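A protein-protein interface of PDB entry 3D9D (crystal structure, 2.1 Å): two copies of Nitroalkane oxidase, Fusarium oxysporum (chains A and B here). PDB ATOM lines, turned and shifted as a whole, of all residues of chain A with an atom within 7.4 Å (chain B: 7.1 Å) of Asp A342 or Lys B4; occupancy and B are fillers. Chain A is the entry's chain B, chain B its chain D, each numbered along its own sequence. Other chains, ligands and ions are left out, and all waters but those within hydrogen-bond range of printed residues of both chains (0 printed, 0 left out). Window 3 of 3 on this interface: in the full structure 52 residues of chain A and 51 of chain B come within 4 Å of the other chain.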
ATOM      1  N   VAL A   1      -4.680  -5.681   9.400  1.00  0.00           N
ATOM      2  CA  VAL A   1      -6.085  -5.456   8.952  1.00  0.00           C
ATOM      3  C   VAL A   1      -6.793  -4.490   9.884  1.00  0.00           C
ATOM      4  O   VAL A   1      -6.647  -4.553  11.116  1.00  0.00           O
ATOM      5  CB  VAL A   1      -6.912  -6.789   8.761  1.00  0.00           C
ATOM      6  CG1 VAL A   1      -6.003  -7.982   8.585  1.00  0.00           C
ATOM      7  CG2 VAL A   1      -7.893  -7.012   9.870  1.00  0.00           C
ATOM      8  N   ASP A   2      -7.565  -3.595   9.288  1.00  0.00           N
ATOM      9  CA  ASP A   2      -8.041  -2.421   9.989  1.00  0.00           C
ATOM     10  C   ASP A   2      -9.371  -1.985   9.405  1.00  0.00           C
ATOM     11  O   ASP A   2      -9.495  -1.872   8.180  1.00  0.00           O
ATOM     12  CB  ASP A   2      -7.008  -1.289   9.821  1.00  0.00           C
ATOM     13  CG  ASP A   2      -7.454   0.000  10.465  1.00  0.00           C
ATOM     14  OD1 ASP A   2      -7.750  -0.032  11.682  1.00  0.00           O
ATOM     15  OD2 ASP A   2      -7.534   1.036   9.756  1.00  0.00           O
ATOM     16  N   LYS A 335     -14.509  -4.744   1.211  1.00  0.00           N
ATOM     17  CA  LYS A 335     -13.518  -5.676   0.738  1.00  0.00           C
ATOM     18  C   LYS A 335     -13.386  -5.636  -0.811  1.00  0.00           C
ATOM     19  O   LYS A 335     -12.262  -5.617  -1.331  1.00  0.00           O
ATOM     20  CB  LYS A 335     -13.805  -7.094   1.230  1.00  0.00           C
ATOM     21  CG  LYS A 335     -12.910  -8.169   0.586  1.00  0.00           C
ATOM     22  CD  LYS A 335     -11.456  -8.026   1.124  1.00  0.00           C
ATOM     23  CE  LYS A 335     -10.510  -9.069   0.551  1.00  0.00           C
ATOM     24  NZ  LYS A 335      -9.117  -8.838   1.091  1.00  0.00           N
ATOM     25  N   ALA A 336     -14.515  -5.606  -1.531  1.00  0.00           N
ATOM     26  CA  ALA A 336     -14.454  -5.586  -2.986  1.00  0.00           C
ATOM     27  C   ALA A 336     -13.791  -4.332  -3.541  1.00  0.00           C
ATOM     28  O   ALA A 336     -12.980  -4.439  -4.459  1.00  0.00           O
ATOM     29  CB  ALA A 336     -15.820  -5.768  -3.621  1.00  0.00           C
ATOM     30  N   VAL A 337     -14.153  -3.154  -3.020  1.00  0.00           N
ATOM     31  CA  VAL A 337     -13.626  -1.918  -3.608  1.00  0.00           C
ATOM     32  C   VAL A 337     -12.146  -1.765  -3.297  1.00  0.00           C
ATOM     33  O   VAL A 337     -11.407  -1.254  -4.114  1.00  0.00           O
ATOM     34  CB  VAL A 337     -14.409  -0.635  -3.199  1.00  0.00           C
ATOM     35  CG1 VAL A 337     -15.855  -0.685  -3.704  1.00  0.00           C
ATOM     36  CG2 VAL A 337     -14.326  -0.372  -1.672  1.00  0.00           C
ATOM     37  N   THR A 338     -11.709  -2.220  -2.127  1.00  0.00           N
ATOM     38  CA  THR A 338     -10.284  -2.204  -1.821  1.00  0.00           C
ATOM     39  C   THR A 338      -9.500  -3.257  -2.624  1.00  0.00           C
ATOM     40  O   THR A 338      -8.338  -3.055  -2.961  1.00  0.00           O
ATOM     41  CB  THR A 338      -9.984  -2.335  -0.309  1.00  0.00           C
ATOM     42  OG1 THR A 338     -10.432  -3.599   0.189  1.00  0.00           O
ATOM     43  CG2 THR A 338     -10.634  -1.247   0.439  1.00  0.00           C
ATOM     44  N   THR A 339     -10.148  -4.375  -2.942  1.00  0.00           N
ATOM     45  CA  THR A 339      -9.533  -5.377  -3.805  1.00  0.00           C
ATOM     46  C   THR A 339      -9.312  -4.754  -5.183  1.00  0.00           C
ATOM     47  O   THR A 339      -8.240  -4.890  -5.772  1.00  0.00           O
ATOM     48  CB  THR A 339     -10.417  -6.654  -3.915  1.00  0.00           C
ATOM     49  OG1 THR A 339     -10.573  -7.240  -2.612  1.00  0.00           O
ATOM     50  CG2 THR A 339      -9.820  -7.672  -4.874  1.00  0.00           C
ATOM     51  N   LEU A 340     -10.333  -4.058  -5.666  1.00  0.00           N
ATOM     52  CA  LEU A 340     -10.291  -3.420  -6.978  1.00  0.00           C
ATOM     53  C   LEU A 340      -9.181  -2.362  -7.069  1.00  0.00           C
ATOM     54  O   LEU A 340      -8.633  -2.147  -8.128  1.00  0.00           O
ATOM     55  CB  LEU A 340     -11.648  -2.799  -7.314  1.00  0.00           C
ATOM     56  CG  LEU A 340     -12.721  -3.723  -7.886  1.00  0.00           C
ATOM     57  CD1 LEU A 340     -14.071  -2.996  -7.896  1.00  0.00           C
ATOM     58  CD2 LEU A 340     -12.322  -4.123  -9.318  1.00  0.00           C
ATOM     59  N   GLU A 341      -8.874  -1.728  -5.940  1.00  0.00           N
ATOM     60  CA  GLU A 341      -7.807  -0.740  -5.846  1.00  0.00           C
ATOM     61  C   GLU A 341      -6.421  -1.346  -5.604  1.00  0.00           C
ATOM     62  O   GLU A 341      -5.436  -0.602  -5.559  1.00  0.00           O
ATOM     63  CB  GLU A 341      -8.093   0.251  -4.717  1.00  0.00           C
ATOM     64  CG  GLU A 341      -9.345   1.084  -4.907  1.00  0.00           C
ATOM     65  CD  GLU A 341      -9.628   1.993  -3.724  1.00  0.00           C
ATOM     66  OE1 GLU A 341     -10.014   3.140  -3.970  1.00  0.00           O
ATOM     67  OE2 GLU A 341      -9.451   1.569  -2.552  1.00  0.00           O
ATOM     68  N   ASP A 342      -6.330  -2.664  -5.415  1.00  0.00           N
ATOM     69  CA  ASP A 342      -5.026  -3.266  -5.104  1.00  0.00           C
ATOM     70  C   ASP A 342      -4.268  -3.467  -6.405  1.00  0.00           C
ATOM     71  O   ASP A 342      -4.680  -4.253  -7.231  1.00  0.00           O
ATOM     72  CB  ASP A 342      -5.172  -4.586  -4.346  1.00  0.00           C
ATOM     73  CG  ASP A 342      -3.850  -5.095  -3.758  1.00  0.00           C
ATOM     74  OD1 ASP A 342      -2.785  -4.992  -4.406  1.00  0.00           O
ATOM     75  OD2 ASP A 342      -3.881  -5.648  -2.638  1.00  0.00           O
ATOM     76  N   GLU A 343      -3.165  -2.752  -6.583  1.00  0.00           N
ATOM     77  CA  GLU A 343      -2.383  -2.832  -7.829  1.00  0.00           C
ATOM     78  C   GLU A 343      -1.590  -4.137  -7.979  1.00  0.00           C
ATOM     79  O   GLU A 343      -1.159  -4.481  -9.084  1.00  0.00           O
ATOM     80  CB  GLU A 343      -1.418  -1.648  -7.909  1.00  0.00           C
ATOM     81  CG  GLU A 343      -2.081  -0.301  -8.186  1.00  0.00           C
ATOM     82  CD  GLU A 343      -1.061   0.840  -8.230  1.00  0.00           C
ATOM     83  OE1 GLU A 343      -0.707   1.276  -9.359  1.00  0.00           O
ATOM     84  OE2 GLU A 343      -0.602   1.278  -7.135  1.00  0.00           O
ATOM     85  N   ALA A 344      -1.383  -4.851  -6.873  1.00  0.00           N
ATOM     86  CA  ALA A 344      -0.677  -6.137  -6.900  1.00  0.00           C
ATOM     87  C   ALA A 344      -1.505  -7.313  -7.435  1.00  0.00           C
ATOM     88  O   ALA A 344      -0.928  -8.321  -7.822  1.00  0.00           O
ATOM     89  CB  ALA A 344      -0.127  -6.479  -5.518  1.00  0.00           C
ATOM     90  N   LEU A 345      -2.833  -7.194  -7.467  1.00  0.00           N
ATOM     91  CA  LEU A 345      -3.694  -8.351  -7.785  1.00  0.00           C
ATOM     92  C   LEU A 345      -4.047  -8.378  -9.249  1.00  0.00           C
ATOM     93  O   LEU A 345      -4.308  -7.337  -9.845  1.00  0.00           O
ATOM     94  CB  LEU A 345      -4.991  -8.363  -6.953  1.00  0.00           C
ATOM     95  CG  LEU A 345      -4.881  -8.299  -5.432  1.00  0.00           C
ATOM     96  CD1 LEU A 345      -6.250  -8.126  -4.825  1.00  0.00           C
ATOM     97  CD2 LEU A 345      -4.191  -9.538  -4.880  1.00  0.00           C
ATOM     98  N   GLU A 346      -4.048  -9.586  -9.804  1.00  0.00           N
ATOM     99  CA  GLU A 346      -4.498  -9.858 -11.162  1.00  0.00           C
ATOM    100  C   GLU A 346      -5.980  -9.541 -11.308  1.00  0.00           C
ATOM    101  O   GLU A 346      -6.753  -9.623 -10.328  1.00  0.00           O
ATOM    102  CB  GLU A 346      -4.368 -11.337 -11.454  1.00  0.00           C
ATOM    103  CG  GLU A 346      -2.968 -11.873 -11.657  1.00  0.00           C
ATOM    104  CD  GLU A 346      -3.016 -13.348 -12.050  1.00  0.00           C
ATOM    105  OE1 GLU A 346      -4.103 -13.812 -12.472  1.00  0.00           O
ATOM    106  OE2 GLU A 346      -1.984 -14.045 -11.922  1.00  0.00           O
ATOM    107  N   LYS A 350      -9.876  -9.550  -8.929  1.00  0.00           N
ATOM    108  CA  LYS A 350     -10.739  -8.387  -8.725  1.00  0.00           C
ATOM    109  C   LYS A 350     -12.143  -8.608  -9.299  1.00  0.00           C
ATOM    110  O   LYS A 350     -13.147  -8.261  -8.656  1.00  0.00           O
ATOM    111  CB  LYS A 350     -10.113  -7.136  -9.363  1.00  0.00           C
ATOM    112  CG  LYS A 350      -8.628  -6.906  -8.954  1.00  0.00           C
ATOM    113  CD  LYS A 350      -8.097  -5.668  -9.616  1.00  0.00           C
ATOM    114  CE  LYS A 350      -6.742  -5.282  -9.057  1.00  0.00           C
ATOM    115  NZ  LYS A 350      -6.454  -3.860  -9.420  1.00  0.00           N
ATOM    116  N   ALA A 425      -7.012 -15.547  -3.318  1.00  0.00           N
ATOM    117  CA  ALA A 425      -5.927 -14.615  -3.695  1.00  0.00           C
ATOM    118  C   ALA A 425      -6.101 -13.189  -3.173  1.00  0.00           C
ATOM    119  O   ALA A 425      -5.131 -12.529  -2.882  1.00  0.00           O
ATOM    120  CB  ALA A 425      -5.698 -14.590  -5.243  1.00  0.00           C
ATOM    121  N   ALA A 426      -7.334 -12.703  -3.084  1.00  0.00           N
ATOM    122  CA  ALA A 426      -7.593 -11.351  -2.588  1.00  0.00           C
ATOM    123  C   ALA A 426      -7.450 -11.287  -1.053  1.00  0.00           C
ATOM    124  O   ALA A 426      -7.394 -10.198  -0.467  1.00  0.00           O
ATOM    125  CB  ALA A 426      -9.000 -10.864  -3.046  1.00  0.00           C
ATOM    126  N   THR A 427      -7.397 -12.452  -0.414  1.00  0.00           N
ATOM    127  CA  THR A 427      -7.260 -12.526   1.045  1.00  0.00           C
ATOM    128  C   THR A 427      -5.862 -12.978   1.469  1.00  0.00           C
ATOM    129  O   THR A 427      -5.209 -12.294   2.234  1.00  0.00           O
ATOM    130  CB  THR A 427      -8.310 -13.449   1.682  1.00  0.00           C
ATOM    131  OG1 THR A 427      -9.599 -12.948   1.350  1.00  0.00           O
ATOM    132  CG2 THR A 427      -8.165 -13.527   3.228  1.00  0.00           C
ATOM    133  N   VAL B   1      -9.267   2.071   6.359  1.00  0.00           N
ATOM    134  CA  VAL B   1      -9.734   0.648   6.272  1.00  0.00           C
ATOM    135  C   VAL B   1      -8.843  -0.184   5.344  1.00  0.00           C
ATOM    136  O   VAL B   1      -8.537   0.205   4.210  1.00  0.00           O
ATOM    137  CB  VAL B   1     -11.279   0.488   5.974  1.00  0.00           C
ATOM    138  CG1 VAL B   1     -12.014   1.821   5.921  1.00  0.00           C
ATOM    139  CG2 VAL B   1     -11.548  -0.369   4.751  1.00  0.00           C
ATOM    140  N   ASP B   2      -8.424  -1.334   5.847  1.00  0.00           N
ATOM    141  CA  ASP B   2      -7.343  -2.062   5.219  1.00  0.00           C
ATOM    142  C   ASP B   2      -7.454  -3.547   5.521  1.00  0.00           C
ATOM    143  O   ASP B   2      -7.718  -3.915   6.657  1.00  0.00           O
ATOM    144  CB  ASP B   2      -6.031  -1.495   5.759  1.00  0.00           C
ATOM    145  CG  ASP B   2      -4.875  -2.321   5.388  1.00  0.00           C
ATOM    146  OD1 ASP B   2      -4.495  -3.167   6.217  1.00  0.00           O
ATOM    147  OD2 ASP B   2      -4.366  -2.158   4.257  1.00  0.00           O
ATOM    148  N   PHE B   3      -7.248  -4.386   4.505  1.00  0.00           N
ATOM    149  CA  PHE B   3      -7.363  -5.833   4.633  1.00  0.00           C
ATOM    150  C   PHE B   3      -6.038  -6.588   4.506  1.00  0.00           C
ATOM    151  O   PHE B   3      -6.007  -7.807   4.628  1.00  0.00           O
ATOM    152  CB  PHE B   3      -8.377  -6.389   3.620  1.00  0.00           C
ATOM    153  CG  PHE B   3      -9.792  -5.924   3.852  1.00  0.00           C
ATOM    154  CD1 PHE B   3     -10.290  -4.815   3.182  1.00  0.00           C
ATOM    155  CD2 PHE B   3     -10.630  -6.593   4.756  1.00  0.00           C
ATOM    156  CE1 PHE B   3     -11.600  -4.368   3.412  1.00  0.00           C
ATOM    157  CE2 PHE B   3     -11.929  -6.154   4.974  1.00  0.00           C
ATOM    158  CZ  PHE B   3     -12.408  -5.037   4.299  1.00  0.00           C
ATOM    159  N   LYS B   4      -4.943  -5.878   4.258  1.00  0.00           N
ATOM    160  CA  LYS B   4      -3.664  -6.547   4.030  1.00  0.00           C
ATOM    161  C   LYS B   4      -3.119  -7.216   5.297  1.00  0.00           C
ATOM    162  O   LYS B   4      -3.287  -6.711   6.416  1.00  0.00           O
ATOM    163  CB  LYS B   4      -2.643  -5.583   3.426  1.00  0.00           C
ATOM    164  CG  LYS B   4      -3.208  -4.789   2.273  1.00  0.00           C
ATOM    165  CD  LYS B   4      -2.127  -4.272   1.333  1.00  0.00           C
ATOM    166  CE  LYS B   4      -2.741  -3.444   0.205  1.00  0.00           C
ATOM    167  NZ  LYS B   4      -1.716  -2.559  -0.443  1.00  0.00           N
ATOM    168  N   LEU B   5      -2.512  -8.380   5.100  1.00  0.00           N
ATOM    169  CA  LEU B   5      -1.939  -9.146   6.177  1.00  0.00           C
ATOM    170  C   LEU B   5      -0.480  -8.752   6.322  1.00  0.00           C
ATOM    171  O   LEU B   5       0.217  -8.514   5.325  1.00  0.00           O
ATOM    172  CB  LEU B   5      -2.078 -10.650   5.910  1.00  0.00           C
ATOM    173  CG  LEU B   5      -3.526 -11.127   5.721  1.00  0.00           C
ATOM    174  CD1 LEU B   5      -3.578 -12.602   5.305  1.00  0.00           C
ATOM    175  CD2 LEU B   5      -4.358 -10.898   6.985  1.00  0.00           C
ATOM    176  N   SER B   6      -0.029  -8.677   7.564  1.00  0.00           N
ATOM    177  CA  SER B   6       1.358  -8.374   7.858  1.00  0.00           C
ATOM    178  C   SER B   6       2.196  -9.636   7.639  1.00  0.00           C
ATOM    179  O   SER B   6       1.651 -10.741   7.515  1.00  0.00           O
ATOM    180  CB  SER B   6       1.473  -7.932   9.304  1.00  0.00           C
ATOM    181  OG  SER B   6       1.200  -9.032  10.159  1.00  0.00           O
ATOM    182  N   GLN B   9       1.277 -12.386  10.188  1.00  0.00           N
ATOM    183  CA  GLN B   9      -0.009 -13.040   9.923  1.00  0.00           C
ATOM    184  C   GLN B   9       0.152 -14.096   8.840  1.00  0.00           C
ATOM    185  O   GLN B   9      -0.377 -15.204   8.978  1.00  0.00           O
ATOM    186  CB  GLN B   9      -1.104 -12.016   9.593  1.00  0.00           C
ATOM    187  CG  GLN B   9      -1.378 -11.116  10.807  1.00  0.00           C
ATOM    188  CD  GLN B   9      -2.241  -9.934  10.520  1.00  0.00           C
ATOM    189  OE1 GLN B   9      -2.177  -9.334   9.453  1.00  0.00           O
ATOM    190  NE2 GLN B   9      -3.058  -9.578  11.484  1.00  0.00           N
ATOM    191  N   TRP B 334     -13.389 -11.438  11.029  1.00  0.00           N
ATOM    192  CA  TRP B 334     -12.285 -10.483  11.181  1.00  0.00           C
ATOM    193  C   TRP B 334     -12.789  -9.149  11.696  1.00  0.00           C
ATOM    194  O   TRP B 334     -12.136  -8.528  12.519  1.00  0.00           O
ATOM    195  CB  TRP B 334     -11.496 -10.276   9.865  1.00  0.00           C
ATOM    196  CG  TRP B 334     -10.677 -11.503   9.425  1.00  0.00           C
ATOM    197  CD1 TRP B 334     -10.795 -12.781   9.889  1.00  0.00           C
ATOM    198  CD2 TRP B 334      -9.678 -11.538   8.409  1.00  0.00           C
ATOM    199  NE1 TRP B 334      -9.917 -13.602   9.236  1.00  0.00           N
ATOM    200  CE2 TRP B 334      -9.222 -12.868   8.317  1.00  0.00           C
ATOM    201  CE3 TRP B 334      -9.112 -10.565   7.574  1.00  0.00           C
ATOM    202  CZ2 TRP B 334      -8.231 -13.268   7.410  1.00  0.00           C
ATOM    203  CZ3 TRP B 334      -8.107 -10.957   6.673  1.00  0.00           C
ATOM    204  CH2 TRP B 334      -7.685 -12.302   6.601  1.00  0.00           C
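The side-chain hydroxyl (OG1) of Thr A339 is in hydrogen-bond range of the backbone carbonyl oxygen (O) of Lys A335, at 2.7 Å.
The backbone NH (N) of Ala A344 is in hydrogen-bond range of the side-chain carboxylate (OD1) of Asp A342 (2.8 Å).
The backbone carbonyl oxygen (O) of Asp A342 is in hydrogen-bond range of the side-chain amino group (NZ) of Lys A350 (2.8 Å).
NZ of Lys A335 is in hydrogen-bond range of O of Ala A426 (2.7 Å).
The backbone carbonyl oxygen of Lys A335 is in hydrogen-bond range of the side-chain hydroxyl of Thr A338 (3.1 Å).
OD1 of Asp B2 sits at hydrogen-bond distance from N of Lys B4, at 3.4 Å.
Val A1 touches Asp B2, and with the chains exchanged Asp A2 touches Val B1.
Asp B2 touches its own counterpart, Asp A2.
2 positions are printed for both chains.
Of the 11 pairs that touch across the chains among the printed residues, 3 have their exchanged pair printed and touching as well.
Among the printed residues, pairs that only touch across the chains: Asp A2 with Val B1 (3.2 Å), Val A1 with Asp B2 (3.2 Å), Thr A338 with Phe B3 (3.2 Å), Thr A427 with Leu B5 (3.5 Å), Lys A335 with Phe B3 (3.5 Å), Thr A427 with Trp B334 (3.6 Å), Val A1 with Leu B5 (3.7 Å), Asp A342 with Lys B4 (3.8 Å) and Val A1 with Phe B3 (3.96 Å).
Of the 18 printed residues of chain A, 6 touch a printed residue of chain B.
Of the 8 printed residues of chain B, 6 touch a printed residue of chain A.
Among the printed residues, 11 pairs touch across the chains.
Of the printed residues of chain B, Asp A342 touches Lys B4.
Of chain A, only Val A1 and Asp A342 come within 4 Å of Lys B4.
Printed residues of chain A within 4 Å of Trp B334: Thr A427 (3.6 Å).
Of the printed residues of chain B, Asp A2 touches Val B1 (3.2 Å) and Asp B2 (2.6 Å).
Printed residues of chain A within 4 Å of Val B1: Asp A2 (3.2 Å).
Thr A339 touches none of the printed residues of chain B.
N of Val A1 lies within hydrogen-bond range of O of Lys B4, at 3.5 Å.
The backbone carbonyl oxygen (O) of Asp A2 sits at hydrogen-bond distance from the backbone NH (N) of Asp B2 (2.6 Å).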
